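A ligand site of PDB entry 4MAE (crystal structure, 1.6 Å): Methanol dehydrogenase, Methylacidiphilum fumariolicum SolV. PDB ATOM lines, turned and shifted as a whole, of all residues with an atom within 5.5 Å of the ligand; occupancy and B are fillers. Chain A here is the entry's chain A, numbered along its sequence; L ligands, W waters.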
ATOM      1  N   GLU A  55      11.670   9.701  -7.021  1.00  0.00           N
ATOM      2  CA  GLU A  55      12.561   9.081  -6.026  1.00  0.00           C
ATOM      3  C   GLU A  55      13.949   8.839  -6.607  1.00  0.00           C
ATOM      4  O   GLU A  55      14.204   9.126  -7.784  1.00  0.00           O
ATOM      5  CB  GLU A  55      11.954   7.780  -5.481  1.00  0.00           C
ATOM      6  CG  GLU A  55      10.787   8.067  -4.564  1.00  0.00           C
ATOM      7  CD  GLU A  55      10.169   6.835  -3.941  1.00  0.00           C
ATOM      8  OE1 GLU A  55       9.144   7.003  -3.244  1.00  0.00           O
ATOM      9  OE2 GLU A  55      10.688   5.714  -4.114  1.00  0.00           O
ATOM     10  N   CYS A 104       1.330  -0.068  -6.016  1.00  0.00           N
ATOM     11  CA  CYS A 104       0.740   0.140  -4.703  1.00  0.00           C
ATOM     12  C   CYS A 104       0.846   1.580  -4.223  1.00  0.00           C
ATOM     13  O   CYS A 104      -0.082   2.133  -3.614  1.00  0.00           O
ATOM     14  CB  CYS A 104       1.380  -0.802  -3.653  1.00  0.00           C
ATOM     15  SG  CYS A 104       3.119  -0.455  -3.164  1.00  0.00           S
ATOM     16  N   CYS A 105       1.987   2.189  -4.509  1.00  0.00           N
ATOM     17  CA  CYS A 105       2.526   3.236  -3.659  1.00  0.00           C
ATOM     18  C   CYS A 105       3.100   4.388  -4.488  1.00  0.00           C
ATOM     19  O   CYS A 105       4.151   4.936  -4.152  1.00  0.00           O
ATOM     20  CB  CYS A 105       3.587   2.604  -2.765  1.00  0.00           C
ATOM     21  SG  CYS A 105       2.990   1.115  -1.847  1.00  0.00           S
ATOM     22  N   ASP A 106       2.375   4.727  -5.553  1.00  0.00           N
ATOM     23  CA  ASP A 106       2.761   5.731  -6.554  1.00  0.00           C
ATOM     24  C   ASP A 106       3.709   5.135  -7.602  1.00  0.00           C
ATOM     25  O   ASP A 106       4.378   4.118  -7.351  1.00  0.00           O
ATOM     26  CB  ASP A 106       3.358   7.002  -5.913  1.00  0.00           C
ATOM     27  CG  ASP A 106       3.361   8.206  -6.853  1.00  0.00           C
ATOM     28  OD1 ASP A 106       2.584   8.243  -7.837  1.00  0.00           O
ATOM     29  OD2 ASP A 106       4.158   9.140  -6.608  1.00  0.00           O
ATOM     30  N   VAL A 108       6.599   5.481  -8.809  1.00  0.00           N
ATOM     31  CA  VAL A 108       7.981   5.937  -8.602  1.00  0.00           C
ATOM     32  C   VAL A 108       8.982   4.948  -9.193  1.00  0.00           C
ATOM     33  O   VAL A 108       8.643   3.794  -9.479  1.00  0.00           O
ATOM     34  CB  VAL A 108       8.283   6.161  -7.113  1.00  0.00           C
ATOM     35  CG1 VAL A 108       7.370   7.253  -6.529  1.00  0.00           C
ATOM     36  CG2 VAL A 108       8.160   4.850  -6.327  1.00  0.00           C
ATOM     37  N   ARG A 110      13.318   4.216  -8.438  1.00  0.00           N
ATOM     38  CA  ARG A 110      14.444   4.624  -7.584  1.00  0.00           C
ATOM     39  C   ARG A 110      15.779   4.821  -8.321  1.00  0.00           C
ATOM     40  O   ARG A 110      16.776   5.196  -7.697  1.00  0.00           O
ATOM     41  CB  ARG A 110      14.585   3.655  -6.410  1.00  0.00           C
ATOM     42  CG  ARG A 110      13.560   3.920  -5.371  1.00  0.00           C
ATOM     43  CD  ARG A 110      13.453   2.891  -4.231  1.00  0.00           C
ATOM     44  NE  ARG A 110      12.074   3.027  -3.791  1.00  0.00           N
ATOM     45  CZ  ARG A 110      11.059   2.266  -4.185  1.00  0.00           C
ATOM     46  NH1 ARG A 110      11.257   1.172  -4.918  1.00  0.00           N
ATOM     47  NH2 ARG A 110       9.837   2.569  -3.803  1.00  0.00           N
ATOM     48  N   THR A 152       5.156  -5.218 -10.334  1.00  0.00           N
ATOM     49  CA  THR A 152       5.746  -4.032 -10.963  1.00  0.00           C
ATOM     50  C   THR A 152       7.206  -3.992 -10.570  1.00  0.00           C
ATOM     51  O   THR A 152       7.647  -4.827  -9.779  1.00  0.00           O
ATOM     52  CB  THR A 152       5.062  -2.744 -10.469  1.00  0.00           C
ATOM     53  OG1 THR A 152       5.061  -2.702  -9.037  1.00  0.00           O
ATOM     54  CG2 THR A 152       3.633  -2.668 -10.998  1.00  0.00           C
ATOM     55  N   THR A 154       9.942  -1.011  -9.142  1.00  0.00           N
ATOM     56  CA  THR A 154      10.234   0.377  -8.761  1.00  0.00           C
ATOM     57  C   THR A 154      11.654   0.593  -8.258  1.00  0.00           C
ATOM     58  O   THR A 154      12.135   1.730  -8.210  1.00  0.00           O
ATOM     59  CB  THR A 154       9.272   0.858  -7.660  1.00  0.00           C
ATOM     60  OG1 THR A 154       9.400   0.009  -6.513  1.00  0.00           O
ATOM     61  CG2 THR A 154       7.808   0.862  -8.162  1.00  0.00           C
ATOM     62  N   VAL A 168      11.685  -7.014  -7.586  1.00  0.00           N
ATOM     63  CA  VAL A 168      10.288  -6.948  -7.972  1.00  0.00           C
ATOM     64  C   VAL A 168       9.466  -6.369  -6.827  1.00  0.00           C
ATOM     65  O   VAL A 168       9.897  -6.404  -5.663  1.00  0.00           O
ATOM     66  CB  VAL A 168       9.761  -8.352  -8.366  1.00  0.00           C
ATOM     67  CG1 VAL A 168       9.684  -9.266  -7.150  1.00  0.00           C
ATOM     68  CG2 VAL A 168       8.411  -8.237  -9.090  1.00  0.00           C
ATOM     69  N   SER A 169       8.315  -5.814  -7.184  1.00  0.00           N
ATOM     70  CA  SER A 169       7.356  -5.268  -6.238  1.00  0.00           C
ATOM     71  C   SER A 169       6.029  -5.991  -6.381  1.00  0.00           C
ATOM     72  O   SER A 169       5.761  -6.619  -7.401  1.00  0.00           O
ATOM     73  CB  SER A 169       7.144  -3.781  -6.502  1.00  0.00           C
ATOM     74  OG  SER A 169       8.340  -3.062  -6.318  1.00  0.00           O
ATOM     75  N   GLY A 170       5.202  -5.889  -5.342  1.00  0.00           N
ATOM     76  CA  GLY A 170       3.909  -6.565  -5.296  1.00  0.00           C
ATOM     77  C   GLY A 170       3.616  -7.323  -4.008  1.00  0.00           C
ATOM     78  O   GLY A 170       2.840  -8.268  -4.011  1.00  0.00           O
ATOM     79  N   GLY A 171       4.210  -6.898  -2.890  1.00  0.00           N
ATOM     80  CA  GLY A 171       3.890  -7.501  -1.596  1.00  0.00           C
ATOM     81  C   GLY A 171       2.440  -7.322  -1.154  1.00  0.00           C
ATOM     82  O   GLY A 171       1.986  -7.990  -0.230  1.00  0.00           O
ATOM     83  N   GLU A 172       1.718  -6.409  -1.815  1.00  0.00           N
ATOM     84  CA  GLU A 172       0.293  -6.219  -1.574  1.00  0.00           C
ATOM     85  C   GLU A 172      -0.569  -6.925  -2.638  1.00  0.00           C
ATOM     86  O   GLU A 172      -1.804  -6.800  -2.636  1.00  0.00           O
ATOM     87  CB  GLU A 172      -0.017  -4.716  -1.505  1.00  0.00           C
ATOM     88  CG  GLU A 172       0.353  -4.073  -0.158  1.00  0.00           C
ATOM     89  CD  GLU A 172       1.863  -4.064   0.150  1.00  0.00           C
ATOM     90  OE1 GLU A 172       2.282  -4.768   1.086  1.00  0.00           O
ATOM     91  OE2 GLU A 172       2.631  -3.322  -0.506  1.00  0.00           O
ATOM     92  N   THR A 236       9.028  -9.367  -1.392  1.00  0.00           N
ATOM     93  CA  THR A 236       9.499  -8.651  -2.563  1.00  0.00           C
ATOM     94  C   THR A 236      10.737  -7.821  -2.208  1.00  0.00           C
ATOM     95  O   THR A 236      11.134  -7.722  -1.038  1.00  0.00           O
ATOM     96  CB  THR A 236       8.373  -7.801  -3.204  1.00  0.00           C
ATOM     97  OG1 THR A 236       7.951  -6.788  -2.289  1.00  0.00           O
ATOM     98  CG2 THR A 236       7.199  -8.700  -3.573  1.00  0.00           C
ATOM     99  N   TRP A 238      12.273  -4.551  -3.442  1.00  0.00           N
ATOM    100  CA  TRP A 238      12.171  -3.258  -4.126  1.00  0.00           C
ATOM    101  C   TRP A 238      13.061  -2.173  -3.517  1.00  0.00           C
ATOM    102  O   TRP A 238      13.051  -1.021  -3.972  1.00  0.00           O
ATOM    103  CB  TRP A 238      10.702  -2.816  -4.133  1.00  0.00           C
ATOM    104  CG  TRP A 238      10.032  -2.812  -2.780  1.00  0.00           C
ATOM    105  CD1 TRP A 238       9.451  -3.871  -2.155  1.00  0.00           C
ATOM    106  CD2 TRP A 238       9.879  -1.691  -1.894  1.00  0.00           C
ATOM    107  NE1 TRP A 238       8.931  -3.486  -0.940  1.00  0.00           N
ATOM    108  CE2 TRP A 238       9.196  -2.158  -0.750  1.00  0.00           C
ATOM    109  CE3 TRP A 238      10.256  -0.354  -1.954  1.00  0.00           C
ATOM    110  CZ2 TRP A 238       8.879  -1.321   0.317  1.00  0.00           C
ATOM    111  CZ3 TRP A 238       9.936   0.475  -0.892  1.00  0.00           C
ATOM    112  CH2 TRP A 238       9.258  -0.018   0.233  1.00  0.00           C
ATOM    113  N   SER A 255      10.270  -7.879   1.597  1.00  0.00           N
ATOM    114  CA  SER A 255       9.020  -7.274   2.063  1.00  0.00           C
ATOM    115  C   SER A 255       8.213  -8.156   3.001  1.00  0.00           C
ATOM    116  O   SER A 255       8.601  -9.279   3.334  1.00  0.00           O
ATOM    117  CB  SER A 255       8.139  -6.902   0.863  1.00  0.00           C
ATOM    118  OG  SER A 255       7.404  -8.019   0.389  1.00  0.00           O
ATOM    119  N   ASN A 256       7.072  -7.605   3.417  1.00  0.00           N
ATOM    120  CA  ASN A 256       6.009  -8.318   4.123  1.00  0.00           C
ATOM    121  C   ASN A 256       5.605  -9.626   3.437  1.00  0.00           C
ATOM    122  O   ASN A 256       5.739  -9.763   2.232  1.00  0.00           O
ATOM    123  CB  ASN A 256       4.787  -7.406   4.207  1.00  0.00           C
ATOM    124  CG  ASN A 256       4.195  -7.091   2.831  1.00  0.00           C
ATOM    125  OD1 ASN A 256       4.823  -6.401   2.013  1.00  0.00           O
ATOM    126  ND2 ASN A 256       2.995  -7.587   2.573  1.00  0.00           N
ATOM    127  N   ASP A 299       2.915  -5.017   8.257  1.00  0.00           N
ATOM    128  CA  ASP A 299       3.498  -4.570   6.978  1.00  0.00           C
ATOM    129  C   ASP A 299       4.854  -3.897   7.203  1.00  0.00           C
ATOM    130  O   ASP A 299       5.144  -2.878   6.581  1.00  0.00           O
ATOM    131  CB  ASP A 299       2.559  -3.629   6.203  1.00  0.00           C
ATOM    132  CG  ASP A 299       3.077  -3.273   4.797  1.00  0.00           C
ATOM    133  OD1 ASP A 299       3.478  -4.179   4.029  1.00  0.00           O
ATOM    134  OD2 ASP A 299       3.076  -2.065   4.458  1.00  0.00           O
ATOM    135  N   ASP A 301       7.888  -4.115   6.002  1.00  0.00           N
ATOM    136  CA  ASP A 301       8.794  -4.559   4.928  1.00  0.00           C
ATOM    137  C   ASP A 301      10.232  -4.399   5.394  1.00  0.00           C
ATOM    138  O   ASP A 301      10.585  -3.409   6.029  1.00  0.00           O
ATOM    139  CB  ASP A 301       8.595  -3.732   3.656  1.00  0.00           C
ATOM    140  CG  ASP A 301       7.272  -4.023   2.967  1.00  0.00           C
ATOM    141  OD1 ASP A 301       6.329  -4.492   3.619  1.00  0.00           O
ATOM    142  OD2 ASP A 301       7.164  -3.783   1.752  1.00  0.00           O
ATOM    143  N   ARG A 326      11.917  -0.696   8.798  1.00  0.00           N
ATOM    144  CA  ARG A 326      10.535  -0.268   8.977  1.00  0.00           C
ATOM    145  C   ARG A 326      10.009  -0.563  10.381  1.00  0.00           C
ATOM    146  O   ARG A 326       9.242   0.224  10.934  1.00  0.00           O
ATOM    147  CB  ARG A 326       9.626  -0.921   7.927  1.00  0.00           C
ATOM    148  CG  ARG A 326       9.886  -0.460   6.489  1.00  0.00           C
ATOM    149  CD  ARG A 326       8.932   0.627   6.059  1.00  0.00           C
ATOM    150  NE  ARG A 326       7.612   0.064   5.822  1.00  0.00           N
ATOM    151  CZ  ARG A 326       7.185  -0.453   4.674  1.00  0.00           C
ATOM    152  NH1 ARG A 326       7.980  -0.461   3.603  1.00  0.00           N
ATOM    153  NH2 ARG A 326       5.949  -0.951   4.583  1.00  0.00           N
ATOM    154  N   SER A 383       2.722   1.312   9.447  1.00  0.00           N
ATOM    155  CA  SER A 383       3.221   0.478   8.357  1.00  0.00           C
ATOM    156  C   SER A 383       4.272   1.165   7.501  1.00  0.00           C
ATOM    157  O   SER A 383       5.104   0.487   6.900  1.00  0.00           O
ATOM    158  CB  SER A 383       2.051   0.011   7.487  1.00  0.00           C
ATOM    159  OG  SER A 383       1.197  -0.801   8.265  1.00  0.00           O
ATOM    160  N   MET A 384       4.253   2.505   7.444  1.00  0.00           N
ATOM    161  CA  MET A 384       5.300   3.263   6.750  1.00  0.00           C
ATOM    162  C   MET A 384       6.648   3.198   7.469  1.00  0.00           C
ATOM    163  O   MET A 384       7.669   3.559   6.918  1.00  0.00           O
ATOM    164  CB  MET A 384       4.871   4.719   6.564  1.00  0.00           C
ATOM    165  CG  MET A 384       3.599   4.868   5.747  1.00  0.00           C
ATOM    166  SD  MET A 384       3.116   6.572   5.512  1.00  0.00           S
ATOM    167  CE  MET A 384       1.661   6.349   4.484  1.00  0.00           C
ATOM    168  N   ASP A 388      10.815   4.628   5.823  1.00  0.00           N
ATOM    169  CA  ASP A 388      10.504   3.837   4.645  1.00  0.00           C
ATOM    170  C   ASP A 388      11.781   3.800   3.786  1.00  0.00           C
ATOM    171  O   ASP A 388      12.898   3.952   4.299  1.00  0.00           O
ATOM    172  CB  ASP A 388       9.286   4.443   3.922  1.00  0.00           C
ATOM    173  CG  ASP A 388       8.494   3.409   3.153  1.00  0.00           C
ATOM    174  OD1 ASP A 388       9.084   2.733   2.294  1.00  0.00           O
ATOM    175  OD2 ASP A 388       7.272   3.285   3.393  1.00  0.00           O
ATOM    176  N   GLN A 389      11.628   3.605   2.476  1.00  0.00           N
ATOM    177  CA  GLN A 389      12.767   3.397   1.579  1.00  0.00           C
ATOM    178  C   GLN A 389      13.855   4.495   1.597  1.00  0.00           C
ATOM    179  O   GLN A 389      15.018   4.207   1.314  1.00  0.00           O
ATOM    180  CB  GLN A 389      12.263   3.168   0.151  1.00  0.00           C
ATOM    181  CG  GLN A 389      11.356   4.273  -0.414  1.00  0.00           C
ATOM    182  CD  GLN A 389      12.142   5.448  -0.952  1.00  0.00           C
ATOM    183  OE1 GLN A 389      13.142   5.275  -1.649  1.00  0.00           O
ATOM    184  NE2 GLN A 389      11.687   6.665  -0.639  1.00  0.00           N
ATOM    185  N   TRP A 467      11.103  12.048   3.655  1.00  0.00           N
ATOM    186  CA  TRP A 467      11.032  11.007   2.628  1.00  0.00           C
ATOM    187  C   TRP A 467      12.137  11.250   1.610  1.00  0.00           C
ATOM    188  O   TRP A 467      11.947  11.047   0.408  1.00  0.00           O
ATOM    189  CB  TRP A 467       9.655  11.031   1.962  1.00  0.00           C
ATOM    190  CG  TRP A 467       9.092   9.667   1.558  1.00  0.00           C
ATOM    191  CD1 TRP A 467       9.257   9.016   0.371  1.00  0.00           C
ATOM    192  CD2 TRP A 467       8.255   8.834   2.369  1.00  0.00           C
ATOM    193  NE1 TRP A 467       8.578   7.810   0.393  1.00  0.00           N
ATOM    194  CE2 TRP A 467       7.960   7.680   1.612  1.00  0.00           C
ATOM    195  CE3 TRP A 467       7.738   8.940   3.658  1.00  0.00           C
ATOM    196  CZ2 TRP A 467       7.157   6.651   2.098  1.00  0.00           C
ATOM    197  CZ3 TRP A 467       6.946   7.916   4.151  1.00  0.00           C
ATOM    198  CH2 TRP A 467       6.664   6.780   3.372  1.00  0.00           C
ATOM    199  N   GLY A 530       5.361  12.603  -4.084  1.00  0.00           N
ATOM    200  CA  GLY A 530       4.649  11.378  -4.353  1.00  0.00           C
ATOM    201  C   GLY A 530       5.085  10.296  -3.387  1.00  0.00           C
ATOM    202  O   GLY A 530       5.331  10.592  -2.219  1.00  0.00           O
ATOM    203  N   GLY A 531       5.212   9.070  -3.880  1.00  0.00           N
ATOM    204  CA  GLY A 531       5.493   7.934  -3.014  1.00  0.00           C
ATOM    205  C   GLY A 531       4.275   7.628  -2.152  1.00  0.00           C
ATOM    206  O   GLY A 531       3.189   8.167  -2.377  1.00  0.00           O
ATOM    207  N   TRP A 532       4.434   6.775  -1.153  1.00  0.00           N
ATOM    208  CA  TRP A 532       3.273   6.266  -0.428  1.00  0.00           C
ATOM    209  C   TRP A 532       2.562   7.356   0.388  1.00  0.00           C
ATOM    210  O   TRP A 532       1.350   7.547   0.243  1.00  0.00           O
ATOM    211  CB  TRP A 532       3.649   5.066   0.438  1.00  0.00           C
ATOM    212  CG  TRP A 532       2.468   4.371   1.062  1.00  0.00           C
ATOM    213  CD1 TRP A 532       1.146   4.478   0.708  1.00  0.00           C
ATOM    214  CD2 TRP A 532       2.519   3.418   2.118  1.00  0.00           C
ATOM    215  NE1 TRP A 532       0.379   3.670   1.497  1.00  0.00           N
ATOM    216  CE2 TRP A 532       1.185   2.997   2.372  1.00  0.00           C
ATOM    217  CE3 TRP A 532       3.553   2.862   2.872  1.00  0.00           C
ATOM    218  CZ2 TRP A 532       0.875   2.073   3.375  1.00  0.00           C
ATOM    219  CZ3 TRP A 532       3.240   1.925   3.858  1.00  0.00           C
ATOM    220  CH2 TRP A 532       1.904   1.539   4.091  1.00  0.00           C
ATOM    221  N   PHE A 533       3.311   8.090   1.207  1.00  0.00           N
ATOM    222  CA  PHE A 533       2.689   9.149   2.009  1.00  0.00           C
ATOM    223  C   PHE A 533       2.128  10.264   1.123  1.00  0.00           C
ATOM    224  O   PHE A 533       1.127  10.877   1.467  1.00  0.00           O
ATOM    225  CB  PHE A 533       3.665   9.712   3.038  1.00  0.00           C
ATOM    226  CG  PHE A 533       3.048  10.741   3.967  1.00  0.00           C
ATOM    227  CD1 PHE A 533       2.460  10.348   5.163  1.00  0.00           C
ATOM    228  CD2 PHE A 533       3.078  12.091   3.648  1.00  0.00           C
ATOM    229  CE1 PHE A 533       1.900  11.291   6.023  1.00  0.00           C
ATOM    230  CE2 PHE A 533       2.521  13.038   4.499  1.00  0.00           C
ATOM    231  CZ  PHE A 533       1.934  12.639   5.682  1.00  0.00           C
HETATM  232  N1  LIG L   1       7.002   2.309  -1.965  1.00  0.00           N
HETATM  233  C1  LIG L   1       6.998   3.473  -1.234  1.00  0.00           C
HETATM  234  C2  LIG L   1       7.383   4.807  -1.757  1.00  0.00           C
HETATM  235  O1  LIG L   1       8.055   4.835  -2.803  1.00  0.00           O
HETATM  236  O2  LIG L   1       7.082   5.840  -1.119  1.00  0.00           O
HETATM  237  C3  LIG L   1       6.605   3.210   0.072  1.00  0.00           C
HETATM  238  C4  LIG L   1       6.338   1.823   0.142  1.00  0.00           C
HETATM  239  C5  LIG L   1       6.608   1.272  -1.195  1.00  0.00           C
HETATM  240  C6  LIG L   1       5.899   0.939   1.260  1.00  0.00           C
HETATM  241  O3  LIG L   1       6.098   1.264   2.443  1.00  0.00           O
HETATM  242  C7  LIG L   1       5.735  -0.500   0.951  1.00  0.00           C
HETATM  243  O4  LIG L   1       5.371  -1.292   1.838  1.00  0.00           O
HETATM  244  C8  LIG L   1       6.016  -0.988  -0.425  1.00  0.00           C
HETATM  245  N2  LIG L   1       5.848  -2.298  -0.618  1.00  0.00           N
HETATM  246  C9  LIG L   1       6.079  -2.865  -1.805  1.00  0.00           C
HETATM  247  C10 LIG L   1       5.877  -4.343  -1.848  1.00  0.00           C
HETATM  248  O5  LIG L   1       5.508  -4.918  -0.789  1.00  0.00           O
HETATM  249  O6  LIG L   1       6.147  -4.982  -2.890  1.00  0.00           O
HETATM  250  C11 LIG L   1       6.514  -2.124  -2.912  1.00  0.00           C
HETATM  251  C12 LIG L   1       6.718  -0.739  -2.847  1.00  0.00           C
HETATM  252  C13 LIG L   1       7.187  -0.047  -4.107  1.00  0.00           C
HETATM  253  O7  LIG L   1       7.473  -0.779  -5.088  1.00  0.00           O
HETATM  254  O8  LIG L   1       7.290   1.199  -4.190  1.00  0.00           O
HETATM  255  C14 LIG L   1       6.470  -0.085  -1.519  1.00  0.00           C
HETATM  256  O   HOH W   1       2.820  -4.190  -3.206  1.00  0.00           O
HETATM  257  O   HOH W   2       4.683  -0.871  -6.930  1.00  0.00           O
HETATM  258  O   HOH W   3       4.445   1.714  -5.965  1.00  0.00           O
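Water W2 lies within hydrogen-bond range of the side-chain hydroxyl of Thr 152 (2.8 Å) and an oxygen (O7) of the ligand (3.3 Å). Water W1 lies within hydrogen-bond range of N of Glu 172 (2.8 Å), N of Gly 171 (3.1 Å), O6 of the ligand (3.4 Å) and SG of Cys 104 (3.7 Å). Water W3 lies within hydrogen-bond range of O of Asp 106 (2.8 Å), N of Cys 105 (2.9 Å), O8 of the ligand (3.4 Å) and SG of Cys 104 (3.8 Å).
An oxygen (O1) of the ligand lies close to the side-chain carboxylate of Glu 55, 2.5 Å away. O7 of the ligand lies within hydrogen-bond range of OG1 of Thr 154. The side-chain carboxylate of Asp 388 lies close to an oxygen (O3) of the ligand. The side-chain hydroxyl (OG1) of Thr 236 sits at hydrogen-bond distance from an oxygen (O6) of the ligand (2.6 Å). The backbone NH (N) of Gly 171 is in hydrogen-bond range of an oxygen (O6) of the ligand (2.7 Å). The side-chain hydroxyl (OG) of Ser 169 is in hydrogen-bond range of an oxygen (O7) of the ligand. The backbone NH of Gly 170 is in hydrogen-bond range of an oxygen (O6) of the ligand (2.8 Å). The guanidinium group (NH1) of Arg 326 is in hydrogen-bond range of an oxygen (O3) of the ligand (2.8 Å). O2 of the ligand lies within hydrogen-bond range of N of Trp 532. An oxygen (O2) of the ligand sits at hydrogen-bond distance from the indole nitrogen of Trp 467, at 2.9 Å. An oxygen (O8) of the ligand is in salt-bridge range of the guanidinium group of Arg 110, 2.9 Å away. A nitrogen (N2) of the ligand sits close to the indole nitrogen (NE1) of Trp 238, at 3.3 Å. O5 of the ligand sits close to OD1 of Asn 256 (3.2 Å).
The side-chain carboxylate of Glu 172 lies close to an oxygen (O5) of the ligand (3.3 Å). O4 of the ligand lies close to OD2 of Asp 301, 3.1 Å away. Merely in contact with the ligand: Gly 531 (3.2 Å), Cys 105 (3.5 Å), Val 108 (3.5 Å), Asp 299 (3.6 Å), Cys 104 (3.6 Å) and Ser 255 (3.7 Å). Along chain A the residues within 4 Å of the ligand span positions 55 to 532. The nearest printed residue that does not touch the ligand is Gln 389 (4.1 Å).
OG1 of Thr 154 lies within hydrogen-bond range of NH1 of Arg 110 (2.7 Å). The backbone NH (N) of Ser 169 lies within hydrogen-bond range of the backbone carbonyl oxygen (O) of Thr 152, at 2.9 Å. The guanidinium group of Arg 326 is in salt-bridge range of the side-chain carboxylate of Asp 299, at 3.1 Å. The backbone carbonyl oxygen of Ser 383 lies within hydrogen-bond range of the guanidinium group of Arg 326. The side-chain amide oxygen (OD1) of Asn 256 lies close to the side-chain carboxylate (OD1) of Asp 301 (2.9 Å). N of Gly 531 is in hydrogen-bond range of OD2 of Asp 106, at 2.9 Å. OE1 of Glu 172 lies close to OD1 of Asn 256 (3.2 Å). The side-chain carboxylate (OD1) of Asp 299 lies close to the side-chain amide oxygen (OD1) of Asn 256, at 3.3 Å.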
